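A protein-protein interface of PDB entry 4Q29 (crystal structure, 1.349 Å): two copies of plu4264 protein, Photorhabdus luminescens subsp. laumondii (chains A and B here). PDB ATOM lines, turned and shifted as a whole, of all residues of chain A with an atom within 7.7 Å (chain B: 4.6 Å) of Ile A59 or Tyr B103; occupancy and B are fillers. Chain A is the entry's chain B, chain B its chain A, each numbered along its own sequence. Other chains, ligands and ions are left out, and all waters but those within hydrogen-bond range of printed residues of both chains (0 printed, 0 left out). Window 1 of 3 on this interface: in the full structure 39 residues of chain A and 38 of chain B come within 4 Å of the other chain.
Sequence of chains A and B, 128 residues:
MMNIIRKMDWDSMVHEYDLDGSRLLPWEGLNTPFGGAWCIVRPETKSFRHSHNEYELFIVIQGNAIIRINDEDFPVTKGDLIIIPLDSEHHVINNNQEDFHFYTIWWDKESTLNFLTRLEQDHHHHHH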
ATOM      1  N   ALA A  37     -16.779  12.810 -22.235  1.00  0.00           N
ATOM      2  CA  ALA A  37     -15.566  12.592 -23.019  1.00  0.00           C
ATOM      3  C   ALA A  37     -15.836  11.648 -24.181  1.00  0.00           C
ATOM      4  O   ALA A  37     -16.505  10.636 -24.032  1.00  0.00           O
ATOM      5  CB  ALA A  37     -14.419  12.022 -22.179  1.00  0.00           C
ATOM      6  N   CYS A  39     -14.076   8.919 -26.237  1.00  0.00           N
ATOM      7  CA  CYS A  39     -13.026   7.963 -25.913  1.00  0.00           C
ATOM      8  C   CYS A  39     -12.747   6.990 -27.050  1.00  0.00           C
ATOM      9  O   CYS A  39     -13.662   6.455 -27.651  1.00  0.00           O
ATOM     10  CB  CYS A  39     -13.439   7.152 -24.661  1.00  0.00           C
ATOM     11  SG  CYS A  39     -13.725   8.035 -23.162  1.00  0.00           S
ATOM     12  N   LEU A  57     -22.674   6.769 -17.956  1.00  0.00           N
ATOM     13  CA  LEU A  57     -23.145   5.889 -19.027  1.00  0.00           C
ATOM     14  C   LEU A  57     -22.271   6.058 -20.240  1.00  0.00           C
ATOM     15  O   LEU A  57     -21.644   7.078 -20.428  1.00  0.00           O
ATOM     16  CB  LEU A  57     -24.592   6.116 -19.372  1.00  0.00           C
ATOM     17  CG  LEU A  57     -24.940   7.479 -19.896  1.00  0.00           C
ATOM     18  CD1 LEU A  57     -24.681   7.635 -21.477  1.00  0.00           C
ATOM     19  CD2 LEU A  57     -26.398   7.675 -19.632  1.00  0.00           C
ATOM     20  N   PHE A  58     -22.244   4.993 -21.047  1.00  0.00           N
ATOM     21  CA  PHE A  58     -21.509   4.973 -22.311  1.00  0.00           C
ATOM     22  C   PHE A  58     -22.510   4.922 -23.456  1.00  0.00           C
ATOM     23  O   PHE A  58     -23.473   4.169 -23.446  1.00  0.00           O
ATOM     24  CB  PHE A  58     -20.633   3.712 -22.465  1.00  0.00           C
ATOM     25  CG  PHE A  58     -19.566   3.487 -21.436  1.00  0.00           C
ATOM     26  CD1 PHE A  58     -19.134   4.489 -20.600  1.00  0.00           C
ATOM     27  CD2 PHE A  58     -18.944   2.232 -21.352  1.00  0.00           C
ATOM     28  CE1 PHE A  58     -18.137   4.255 -19.681  1.00  0.00           C
ATOM     29  CE2 PHE A  58     -17.938   2.005 -20.439  1.00  0.00           C
ATOM     30  CZ  PHE A  58     -17.550   3.005 -19.585  1.00  0.00           C
ATOM     31  N   ILE A  59     -22.181   5.694 -24.480  1.00  0.00           N
ATOM     32  CA  ILE A  59     -22.874   5.660 -25.771  1.00  0.00           C
ATOM     33  C   ILE A  59     -21.866   5.115 -26.804  1.00  0.00           C
ATOM     34  O   ILE A  59     -20.832   5.731 -27.045  1.00  0.00           O
ATOM     35  CB  ILE A  59     -23.290   7.054 -26.147  1.00  0.00           C
ATOM     36  CG1 ILE A  59     -24.258   7.572 -25.098  1.00  0.00           C
ATOM     37  CG2 ILE A  59     -23.918   7.094 -27.566  1.00  0.00           C
ATOM     38  CD1 ILE A  59     -24.537   8.970 -25.222  1.00  0.00           C
ATOM     39  N   VAL A  60     -22.173   3.940 -27.345  1.00  0.00           N
ATOM     40  CA  VAL A  60     -21.209   3.254 -28.226  1.00  0.00           C
ATOM     41  C   VAL A  60     -21.325   3.783 -29.662  1.00  0.00           C
ATOM     42  O   VAL A  60     -22.384   3.777 -30.247  1.00  0.00           O
ATOM     43  CB  VAL A  60     -21.409   1.761 -28.152  1.00  0.00           C
ATOM     44  CG1 VAL A  60     -20.415   1.061 -29.083  1.00  0.00           C
ATOM     45  CG2 VAL A  60     -21.229   1.233 -26.722  1.00  0.00           C
ATOM     46  N   ILE A  61     -20.212   4.305 -30.127  1.00  0.00           N
ATOM     47  CA  ILE A  61     -20.187   5.054 -31.391  1.00  0.00           C
ATOM     48  C   ILE A  61     -19.658   4.249 -32.573  1.00  0.00           C
ATOM     49  O   ILE A  61     -20.276   4.355 -33.631  1.00  0.00           O
ATOM     50  CB  ILE A  61     -19.380   6.334 -31.196  1.00  0.00           C
ATOM     51  CG1 ILE A  61     -20.190   7.307 -30.309  1.00  0.00           C
ATOM     52  CG2 ILE A  61     -18.980   6.974 -32.523  1.00  0.00           C
ATOM     53  CD1 ILE A  61     -19.413   8.567 -29.914  1.00  0.00           C
ATOM     54  N   GLN A  62     -18.569   3.511 -32.426  1.00  0.00           N
ATOM     55  CA  GLN A  62     -18.012   2.823 -33.565  1.00  0.00           C
ATOM     56  C   GLN A  62     -17.159   1.687 -33.102  1.00  0.00           C
ATOM     57  O   GLN A  62     -16.468   1.740 -32.092  1.00  0.00           O
ATOM     58  CB  GLN A  62     -17.262   3.885 -34.324  1.00  0.00           C
ATOM     59  CG  GLN A  62     -17.521   3.838 -35.703  1.00  0.00           C
ATOM     60  CD  GLN A  62     -16.349   3.438 -36.207  1.00  0.00           C
ATOM     61  OE1 GLN A  62     -16.168   2.211 -36.505  1.00  0.00           O
ATOM     62  NE2 GLN A  62     -15.431   4.401 -36.405  1.00  0.00           N
ATOM     63  N   THR A  77     -21.659  -2.753 -29.545  1.00  0.00           N
ATOM     64  CA  THR A  77     -21.471  -2.262 -30.885  1.00  0.00           C
ATOM     65  C   THR A  77     -22.257  -0.983 -31.067  1.00  0.00           C
ATOM     66  O   THR A  77     -22.959  -0.529 -30.160  1.00  0.00           O
ATOM     67  CB  THR A  77     -21.872  -3.327 -31.912  1.00  0.00           C
ATOM     68  OG1 THR A  77     -21.004  -3.224 -33.044  1.00  0.00           O
ATOM     69  CG2 THR A  77     -23.341  -3.236 -32.311  1.00  0.00           C
ATOM     70  N   LYS A  78     -22.120  -0.364 -32.220  1.00  0.00           N
ATOM     71  CA  LYS A  78     -22.685   0.981 -32.497  1.00  0.00           C
ATOM     72  C   LYS A  78     -24.134   1.042 -32.134  1.00  0.00           C
ATOM     73  O   LYS A  78     -24.922   0.238 -32.524  1.00  0.00           O
ATOM     74  CB  LYS A  78     -22.543   1.300 -34.019  1.00  0.00           C
ATOM     75  CG  LYS A  78     -23.343   2.526 -34.621  1.00  0.00           C
ATOM     76  CD  LYS A  78     -23.445   2.585 -36.210  1.00  0.00           C
ATOM     77  CE  LYS A  78     -23.781   3.958 -36.658  1.00  0.00           C
ATOM     78  NZ  LYS A  78     -24.123   4.001 -38.163  1.00  0.00           N
ATOM     79  N   GLY A  79     -24.470   2.057 -31.326  1.00  0.00           N
ATOM     80  CA  GLY A  79     -25.843   2.292 -30.903  1.00  0.00           C
ATOM     81  C   GLY A  79     -26.156   1.787 -29.516  1.00  0.00           C
ATOM     82  O   GLY A  79     -27.144   2.240 -28.914  1.00  0.00           O
ATOM     83  N   ASP A  80     -25.377   0.875 -28.994  1.00  0.00           N
ATOM     84  CA  ASP A  80     -25.625   0.346 -27.653  1.00  0.00           C
ATOM     85  C   ASP A  80     -25.342   1.399 -26.587  1.00  0.00           C
ATOM     86  O   ASP A  80     -24.476   2.233 -26.718  1.00  0.00           O
ATOM     87  CB  ASP A  80     -24.756  -0.865 -27.377  1.00  0.00           C
ATOM     88  CG  ASP A  80     -25.079  -2.060 -28.288  1.00  0.00           C
ATOM     89  OD1 ASP A  80     -26.141  -2.104 -28.922  1.00  0.00           O
ATOM     90  OD2 ASP A  80     -24.250  -3.005 -28.296  1.00  0.00           O
ATOM     91  N   LEU A  81     -26.172   1.339 -25.541  1.00  0.00           N
ATOM     92  CA  LEU A  81     -26.043   2.171 -24.333  1.00  0.00           C
ATOM     93  C   LEU A  81     -25.756   1.259 -23.168  1.00  0.00           C
ATOM     94  O   LEU A  81     -26.330   0.194 -23.035  1.00  0.00           O
ATOM     95  CB  LEU A  81     -27.341   2.943 -24.047  1.00  0.00           C
ATOM     96  CG  LEU A  81     -27.628   4.327 -24.671  1.00  0.00           C
ATOM     97  CD1 LEU A  81     -26.496   4.869 -25.519  1.00  0.00           C
ATOM     98  CD2 LEU A  81     -28.963   4.362 -25.419  1.00  0.00           C
ATOM     99  N   ILE A  82     -24.846   1.719 -22.316  1.00  0.00           N
ATOM    100  CA  ILE A  82     -24.421   1.034 -21.105  1.00  0.00           C
ATOM    101  C   ILE A  82     -24.525   1.988 -19.946  1.00  0.00           C
ATOM    102  O   ILE A  82     -23.961   3.052 -20.007  1.00  0.00           O
ATOM    103  CB  ILE A  82     -22.939   0.676 -21.182  1.00  0.00           C
ATOM    104  CG1 ILE A  82     -22.658  -0.238 -22.375  1.00  0.00           C
ATOM    105  CG2 ILE A  82     -22.477   0.071 -19.882  1.00  0.00           C
ATOM    106  CD1 ILE A  82     -22.963  -1.654 -22.141  1.00  0.00           C
ATOM    107  N   ILE A  83     -25.195   1.560 -18.890  1.00  0.00           N
ATOM    108  CA  ILE A  83     -25.227   2.323 -17.632  1.00  0.00           C
ATOM    109  C   ILE A  83     -24.309   1.586 -16.687  1.00  0.00           C
ATOM    110  O   ILE A  83     -24.523   0.376 -16.430  1.00  0.00           O
ATOM    111  CB  ILE A  83     -26.633   2.339 -17.039  1.00  0.00           C
ATOM    112  CG1 ILE A  83     -27.677   2.858 -18.026  1.00  0.00           C
ATOM    113  CG2 ILE A  83     -26.654   3.157 -15.739  1.00  0.00           C
ATOM    114  CD1 ILE A  83     -27.356   4.120 -18.765  1.00  0.00           C
ATOM    115  N   PHE A 100     -12.082   1.437 -31.259  1.00  0.00           N
ATOM    116  CA  PHE A 100     -13.401   1.417 -30.612  1.00  0.00           C
ATOM    117  C   PHE A 100     -13.687   2.794 -30.026  1.00  0.00           C
ATOM    118  O   PHE A 100     -12.928   3.287 -29.193  1.00  0.00           O
ATOM    119  CB  PHE A 100     -13.465   0.360 -29.502  1.00  0.00           C
ATOM    120  CG  PHE A 100     -14.793   0.337 -28.807  1.00  0.00           C
ATOM    121  CD1 PHE A 100     -15.890  -0.165 -29.439  1.00  0.00           C
ATOM    122  CD2 PHE A 100     -14.940   0.831 -27.496  1.00  0.00           C
ATOM    123  CE1 PHE A 100     -17.122  -0.173 -28.821  1.00  0.00           C
ATOM    124  CE2 PHE A 100     -16.188   0.804 -26.875  1.00  0.00           C
ATOM    125  CZ  PHE A 100     -17.257   0.330 -27.501  1.00  0.00           C
ATOM    126  N   HIS A 101     -14.767   3.406 -30.499  1.00  0.00           N
ATOM    127  CA  HIS A 101     -15.146   4.759 -30.046  1.00  0.00           C
ATOM    128  C   HIS A 101     -16.420   4.701 -29.204  1.00  0.00           C
ATOM    129  O   HIS A 101     -17.389   4.051 -29.557  1.00  0.00           O
ATOM    130  CB  HIS A 101     -15.457   5.709 -31.200  1.00  0.00           C
ATOM    131  CG  HIS A 101     -14.310   6.009 -32.109  1.00  0.00           C
ATOM    132  ND1 HIS A 101     -13.843   7.283 -32.298  1.00  0.00           N
ATOM    133  CD2 HIS A 101     -13.622   5.215 -32.986  1.00  0.00           C
ATOM    134  CE1 HIS A 101     -12.872   7.264 -33.202  1.00  0.00           C
ATOM    135  NE2 HIS A 101     -12.742   6.022 -33.639  1.00  0.00           N
ATOM    136  N   PHE A 102     -16.420   5.469 -28.096  1.00  0.00           N
ATOM    137  CA  PHE A 102     -17.630   5.627 -27.273  1.00  0.00           C
ATOM    138  C   PHE A 102     -17.541   6.984 -26.630  1.00  0.00           C
ATOM    139  O   PHE A 102     -16.479   7.536 -26.431  1.00  0.00           O
ATOM    140  CB  PHE A 102     -17.806   4.491 -26.268  1.00  0.00           C
ATOM    141  CG  PHE A 102     -16.789   4.446 -25.166  1.00  0.00           C
ATOM    142  CD1 PHE A 102     -15.523   3.936 -25.371  1.00  0.00           C
ATOM    143  CD2 PHE A 102     -17.132   4.862 -23.868  1.00  0.00           C
ATOM    144  CE1 PHE A 102     -14.619   3.878 -24.355  1.00  0.00           C
ATOM    145  CE2 PHE A 102     -16.227   4.796 -22.859  1.00  0.00           C
ATOM    146  CZ  PHE A 102     -14.972   4.301 -23.077  1.00  0.00           C
ATOM    147  N   TYR A 103     -18.730   7.492 -26.262  1.00  0.00           N
ATOM    148  CA  TYR A 103     -18.826   8.752 -25.497  1.00  0.00           C
ATOM    149  C   TYR A 103     -19.316   8.427 -24.111  1.00  0.00           C
ATOM    150  O   TYR A 103     -20.327   7.769 -23.989  1.00  0.00           O
ATOM    151  CB  TYR A 103     -19.806   9.724 -26.167  1.00  0.00           C
ATOM    152  CG  TYR A 103     -19.454  11.156 -25.816  1.00  0.00           C
ATOM    153  CD1 TYR A 103     -19.921  11.756 -24.656  1.00  0.00           C
ATOM    154  CD2 TYR A 103     -18.620  11.910 -26.609  1.00  0.00           C
ATOM    155  CE1 TYR A 103     -19.524  13.009 -24.319  1.00  0.00           C
ATOM    156  CE2 TYR A 103     -18.230  13.170 -26.297  1.00  0.00           C
ATOM    157  CZ  TYR A 103     -18.693  13.722 -25.115  1.00  0.00           C
ATOM    158  OH  TYR A 103     -18.274  14.986 -24.740  1.00  0.00           O
ATOM    159  N   THR A 104     -18.600   8.904 -23.088  1.00  0.00           N
ATOM    160  CA  THR A 104     -19.032   8.738 -21.709  1.00  0.00           C
ATOM    161  C   THR A 104     -19.559  10.068 -21.170  1.00  0.00           C
ATOM    162  O   THR A 104     -19.028  11.115 -21.420  1.00  0.00           O
ATOM    163  CB  THR A 104     -17.908   8.239 -20.802  1.00  0.00           C
ATOM    164  OG1 THR A 104     -18.461   8.172 -19.479  1.00  0.00           O
ATOM    165  CG2 THR A 104     -16.689   9.143 -20.817  1.00  0.00           C
ATOM    166  N   ILE A 105     -20.654   9.954 -20.421  1.00  0.00           N
ATOM    167  CA  ILE A 105     -21.289  11.060 -19.683  1.00  0.00           C
ATOM    168  C   ILE A 105     -21.341  10.618 -18.223  1.00  0.00           C
ATOM    169  O   ILE A 105     -21.771   9.534 -17.919  1.00  0.00           O
ATOM    170  CB  ILE A 105     -22.670  11.367 -20.237  1.00  0.00           C
ATOM    171  CG1 ILE A 105     -22.580  11.830 -21.704  1.00  0.00           C
ATOM    172  CG2 ILE A 105     -23.359  12.370 -19.361  1.00  0.00           C
ATOM    173  CD1 ILE A 105     -22.064  13.225 -21.874  1.00  0.00           C
ATOM    174  N   LEU B  24     -33.264   7.984 -24.708  1.00  0.00           N
ATOM    175  CA  LEU B  24     -32.674   7.340 -23.524  1.00  0.00           C
ATOM    176  C   LEU B  24     -33.717   6.928 -22.494  1.00  0.00           C
ATOM    177  O   LEU B  24     -33.698   5.827 -21.969  1.00  0.00           O
ATOM    178  CB  LEU B  24     -31.655   8.283 -22.911  1.00  0.00           C
ATOM    179  CG  LEU B  24     -31.245   8.092 -21.443  1.00  0.00           C
ATOM    180  CD1 LEU B  24     -31.051   6.679 -20.989  1.00  0.00           C
ATOM    181  CD2 LEU B  24     -30.015   8.901 -21.118  1.00  0.00           C
ATOM    182  N   GLY B  36     -32.013  12.562 -23.419  1.00  0.00           N
ATOM    183  CA  GLY B  36     -31.288  12.518 -24.664  1.00  0.00           C
ATOM    184  C   GLY B  36     -31.857  11.505 -25.605  1.00  0.00           C
ATOM    185  O   GLY B  36     -32.797  10.792 -25.364  1.00  0.00           O
ATOM    186  N   ALA B  37     -31.187  11.432 -26.762  1.00  0.00           N
ATOM    187  CA  ALA B  37     -31.648  10.579 -27.859  1.00  0.00           C
ATOM    188  C   ALA B  37     -30.555  10.407 -28.887  1.00  0.00           C
ATOM    189  O   ALA B  37     -29.832  11.315 -29.220  1.00  0.00           O
ATOM    190  CB  ALA B  37     -32.866  11.143 -28.531  1.00  0.00           C
ATOM    191  N   TRP B  38     -30.539   9.180 -29.389  1.00  0.00           N
ATOM    192  CA  TRP B  38     -29.758   8.888 -30.630  1.00  0.00           C
ATOM    193  C   TRP B  38     -30.657   9.207 -31.810  1.00  0.00           C
ATOM    194  O   TRP B  38     -31.729   8.678 -31.920  1.00  0.00           O
ATOM    195  CB  TRP B  38     -29.353   7.404 -30.675  1.00  0.00           C
ATOM    196  CG  TRP B  38     -28.381   7.043 -31.813  1.00  0.00           C
ATOM    197  CD1 TRP B  38     -28.597   7.186 -33.170  1.00  0.00           C
ATOM    198  CD2 TRP B  38     -27.078   6.532 -31.645  1.00  0.00           C
ATOM    199  NE1 TRP B  38     -27.484   6.743 -33.828  1.00  0.00           N
ATOM    200  CE2 TRP B  38     -26.544   6.325 -32.939  1.00  0.00           C
ATOM    201  CE3 TRP B  38     -26.306   6.156 -30.541  1.00  0.00           C
ATOM    202  CZ2 TRP B  38     -25.271   5.827 -33.138  1.00  0.00           C
ATOM    203  CZ3 TRP B  38     -25.056   5.663 -30.742  1.00  0.00           C
ATOM    204  CH2 TRP B  38     -24.538   5.492 -32.038  1.00  0.00           C
ATOM    205  N   LEU B  57     -27.086  19.899 -26.301  1.00  0.00           N
ATOM    206  CA  LEU B  57     -25.781  19.627 -26.908  1.00  0.00           C
ATOM    207  C   LEU B  57     -25.945  18.484 -27.915  1.00  0.00           C
ATOM    208  O   LEU B  57     -26.605  17.497 -27.621  1.00  0.00           O
ATOM    209  CB  LEU B  57     -24.736  19.210 -25.843  1.00  0.00           C
ATOM    210  CG  LEU B  57     -23.266  18.944 -26.182  1.00  0.00           C
ATOM    211  CD1 LEU B  57     -22.564  20.230 -26.573  1.00  0.00           C
ATOM    212  CD2 LEU B  57     -22.574  18.279 -24.985  1.00  0.00           C
ATOM    213  N   PHE B  58     -25.308  18.618 -29.083  1.00  0.00           N
ATOM    214  CA  PHE B  58     -25.228  17.526 -30.050  1.00  0.00           C
ATOM    215  C   PHE B  58     -23.801  16.987 -30.048  1.00  0.00           C
ATOM    216  O   PHE B  58     -22.834  17.745 -30.137  1.00  0.00           O
ATOM    217  CB  PHE B  58     -25.493  17.963 -31.500  1.00  0.00           C
ATOM    218  CG  PHE B  58     -26.865  18.463 -31.812  1.00  0.00           C
ATOM    219  CD1 PHE B  58     -27.943  18.350 -30.955  1.00  0.00           C
ATOM    220  CD2 PHE B  58     -27.058  19.052 -33.057  1.00  0.00           C
ATOM    221  CE1 PHE B  58     -29.177  18.803 -31.329  1.00  0.00           C
ATOM    222  CE2 PHE B  58     -28.272  19.482 -33.447  1.00  0.00           C
ATOM    223  CZ  PHE B  58     -29.334  19.365 -32.610  1.00  0.00           C
ATOM    224  N   ILE B  59     -23.728  15.668 -30.012  1.00  0.00           N
ATOM    225  CA  ILE B  59     -22.484  14.915 -30.205  1.00  0.00           C
ATOM    226  C   ILE B  59     -22.623  14.213 -31.595  1.00  0.00           C
ATOM    227  O   ILE B  59     -23.467  13.355 -31.770  1.00  0.00           O
ATOM    228  CB  ILE B  59     -22.299  13.847 -29.115  1.00  0.00           C
ATOM    229  CG1 ILE B  59     -22.269  14.470 -27.699  1.00  0.00           C
ATOM    230  CG2 ILE B  59     -21.046  12.983 -29.381  1.00  0.00           C
ATOM    231  CD1 ILE B  59     -22.600  13.477 -26.603  1.00  0.00           C
ATOM    232  N   ILE B  61     -21.970  11.811 -34.466  1.00  0.00           N
ATOM    233  CA  ILE B  61     -21.490  10.418 -34.465  1.00  0.00           C
ATOM    234  C   ILE B  61     -20.980   9.944 -35.841  1.00  0.00           C
ATOM    235  O   ILE B  61     -19.884   9.388 -35.902  1.00  0.00           O
ATOM    236  CB  ILE B  61     -22.628   9.534 -33.873  1.00  0.00           C
ATOM    237  CG1 ILE B  61     -22.770   9.826 -32.365  1.00  0.00           C
ATOM    238  CG2 ILE B  61     -22.454   8.036 -34.158  1.00  0.00           C
ATOM    239  CD1 ILE B  61     -23.912   9.163 -31.743  1.00  0.00           C
ATOM    240  N   PHE B 102     -26.352  11.525 -34.763  1.00  0.00           N
ATOM    241  CA  PHE B 102     -25.877  12.372 -33.671  1.00  0.00           C
ATOM    242  C   PHE B 102     -26.657  11.963 -32.450  1.00  0.00           C
ATOM    243  O   PHE B 102     -27.734  11.446 -32.501  1.00  0.00           O
ATOM    244  CB  PHE B 102     -25.999  13.865 -33.998  1.00  0.00           C
ATOM    245  CG  PHE B 102     -27.397  14.368 -34.128  1.00  0.00           C
ATOM    246  CD1 PHE B 102     -28.137  14.244 -35.283  1.00  0.00           C
ATOM    247  CD2 PHE B 102     -27.969  15.102 -33.068  1.00  0.00           C
ATOM    248  CE1 PHE B 102     -29.400  14.745 -35.378  1.00  0.00           C
ATOM    249  CE2 PHE B 102     -29.228  15.600 -33.170  1.00  0.00           C
ATOM    250  CZ  PHE B 102     -29.954  15.434 -34.311  1.00  0.00           C
ATOM    251  N   TYR B 103     -26.033  12.258 -31.299  1.00  0.00           N
ATOM    252  CA  TYR B 103     -26.679  12.121 -29.998  1.00  0.00           C
ATOM    253  C   TYR B 103     -26.974  13.513 -29.457  1.00  0.00           C
ATOM    254  O   TYR B 103     -26.165  14.402 -29.539  1.00  0.00           O
ATOM    255  CB  TYR B 103     -25.793  11.312 -29.048  1.00  0.00           C
ATOM    256  CG  TYR B 103     -26.629  10.539 -28.010  1.00  0.00           C
ATOM    257  CD1 TYR B 103     -27.068   9.276 -28.215  1.00  0.00           C
ATOM    258  CD2 TYR B 103     -27.073  11.163 -26.832  1.00  0.00           C
ATOM    259  CE1 TYR B 103     -27.900   8.593 -27.340  1.00  0.00           C
ATOM    260  CE2 TYR B 103     -27.879  10.495 -25.958  1.00  0.00           C
ATOM    261  CZ  TYR B 103     -28.323   9.251 -26.221  1.00  0.00           C
ATOM    262  OH  TYR B 103     -29.150   8.635 -25.325  1.00  0.00           O
ATOM    263  N   THR B 104     -28.205  13.676 -29.020  1.00  0.00           N
ATOM    264  CA  THR B 104     -28.625  14.936 -28.364  1.00  0.00           C
ATOM    265  C   THR B 104     -28.795  14.662 -26.868  1.00  0.00           C
ATOM    266  O   THR B 104     -29.339  13.667 -26.458  1.00  0.00           O
ATOM    267  CB  THR B 104     -29.935  15.533 -28.959  1.00  0.00           C
ATOM    268  OG1 THR B 104     -30.327  16.675 -28.159  1.00  0.00           O
ATOM    269  CG2 THR B 104     -31.116  14.544 -28.986  1.00  0.00           C
ATOM    270  N   ILE B 105     -28.276  15.587 -26.073  1.00  0.00           N
ATOM    271  CA  ILE B 105     -28.518  15.630 -24.644  1.00  0.00           C
ATOM    272  C   ILE B 105     -29.087  17.000 -24.318  1.00  0.00           C
ATOM    273  O   ILE B 105     -28.572  18.009 -24.709  1.00  0.00           O
ATOM    274  CB  ILE B 105     -27.262  15.322 -23.884  1.00  0.00           C
ATOM    275  CG1 ILE B 105     -26.849  13.863 -24.160  1.00  0.00           C
ATOM    276  CG2 ILE B 105     -27.458  15.612 -22.395  1.00  0.00           C
ATOM    277  CD1 ILE B 105     -25.529  13.575 -23.757  1.00  0.00           C
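The backbone NH (N) of Ile A61 sits at hydrogen-bond distance from the backbone carbonyl oxygen (O) of His A101 (2.9 Å). N of Leu B57 sits at hydrogen-bond distance from O of Ile B105. N of Ile B59 lies within hydrogen-bond range of O of Tyr B103 (2.8 Å). O of Asp A80 is in hydrogen-bond range of N of Val A60 (2.9 Å). N of Gly A79 lies within hydrogen-bond range of O of Val A60, 2.9 Å away. O of Tyr A103 lies within hydrogen-bond range of N of Ile A59, 2.8 Å away.
Hydrophobic or aromatic side chains of chain A within 4 Å of the printed part of chain B: Ile A59, Ile A61, Tyr A103 and Ile A105. Hydrophobic or aromatic side chains of chain B that line the printed part of chain A: Trp B38, Ile B59, Ile B61, Tyr B103 and Ile B105. Among the printed residues, no Asp or Glu carboxylate lies within 4 Å of a Lys or Arg side-chain nitrogen of the other chain.
Trp B38 touches Ile A59. Ile A59 touches Tyr B103 (CD1 to CD2, 3.7 Å). CH2 of Trp B38 touches O of Val A60, at 3.3 Å. Ile A61 touches Ile B61 (CG2 to CG2, 3.98 Å). Trp B38 touches Gly A79 (CZ3 to CA, 3.5 Å). Tyr A103 touches Ile B59. Ile A105 touches Ile B105.
Ile A59 touches Tyr B103, and with the chains exchanged Tyr A103 touches Ile B59. Ile A61 touches its own counterpart, Ile B61. Ile A105 touches its own counterpart, Ile B105. Positions printed for both chains: 37, 57, 58, 59, 61, 102, 103, 104 and 105.
Ile A59 touches just these residues of chain B: Trp B38 and Tyr B103. Tyr B103 touches just one residue of chain A: Ile A59 (3.7 Å). Of the printed residues of chain B, Val A60 touches Trp B38. Of the printed residues of chain B, Tyr A103 touches Ile B59. Thr A104 touches none of the printed residues of chain B. The nearest printed residue of chain B that does not touch Ile A59 is Ile B61 (4.7 Å). The nearest residue of chain A that does not touch Tyr B103 is Leu A81 (4.3 Å).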
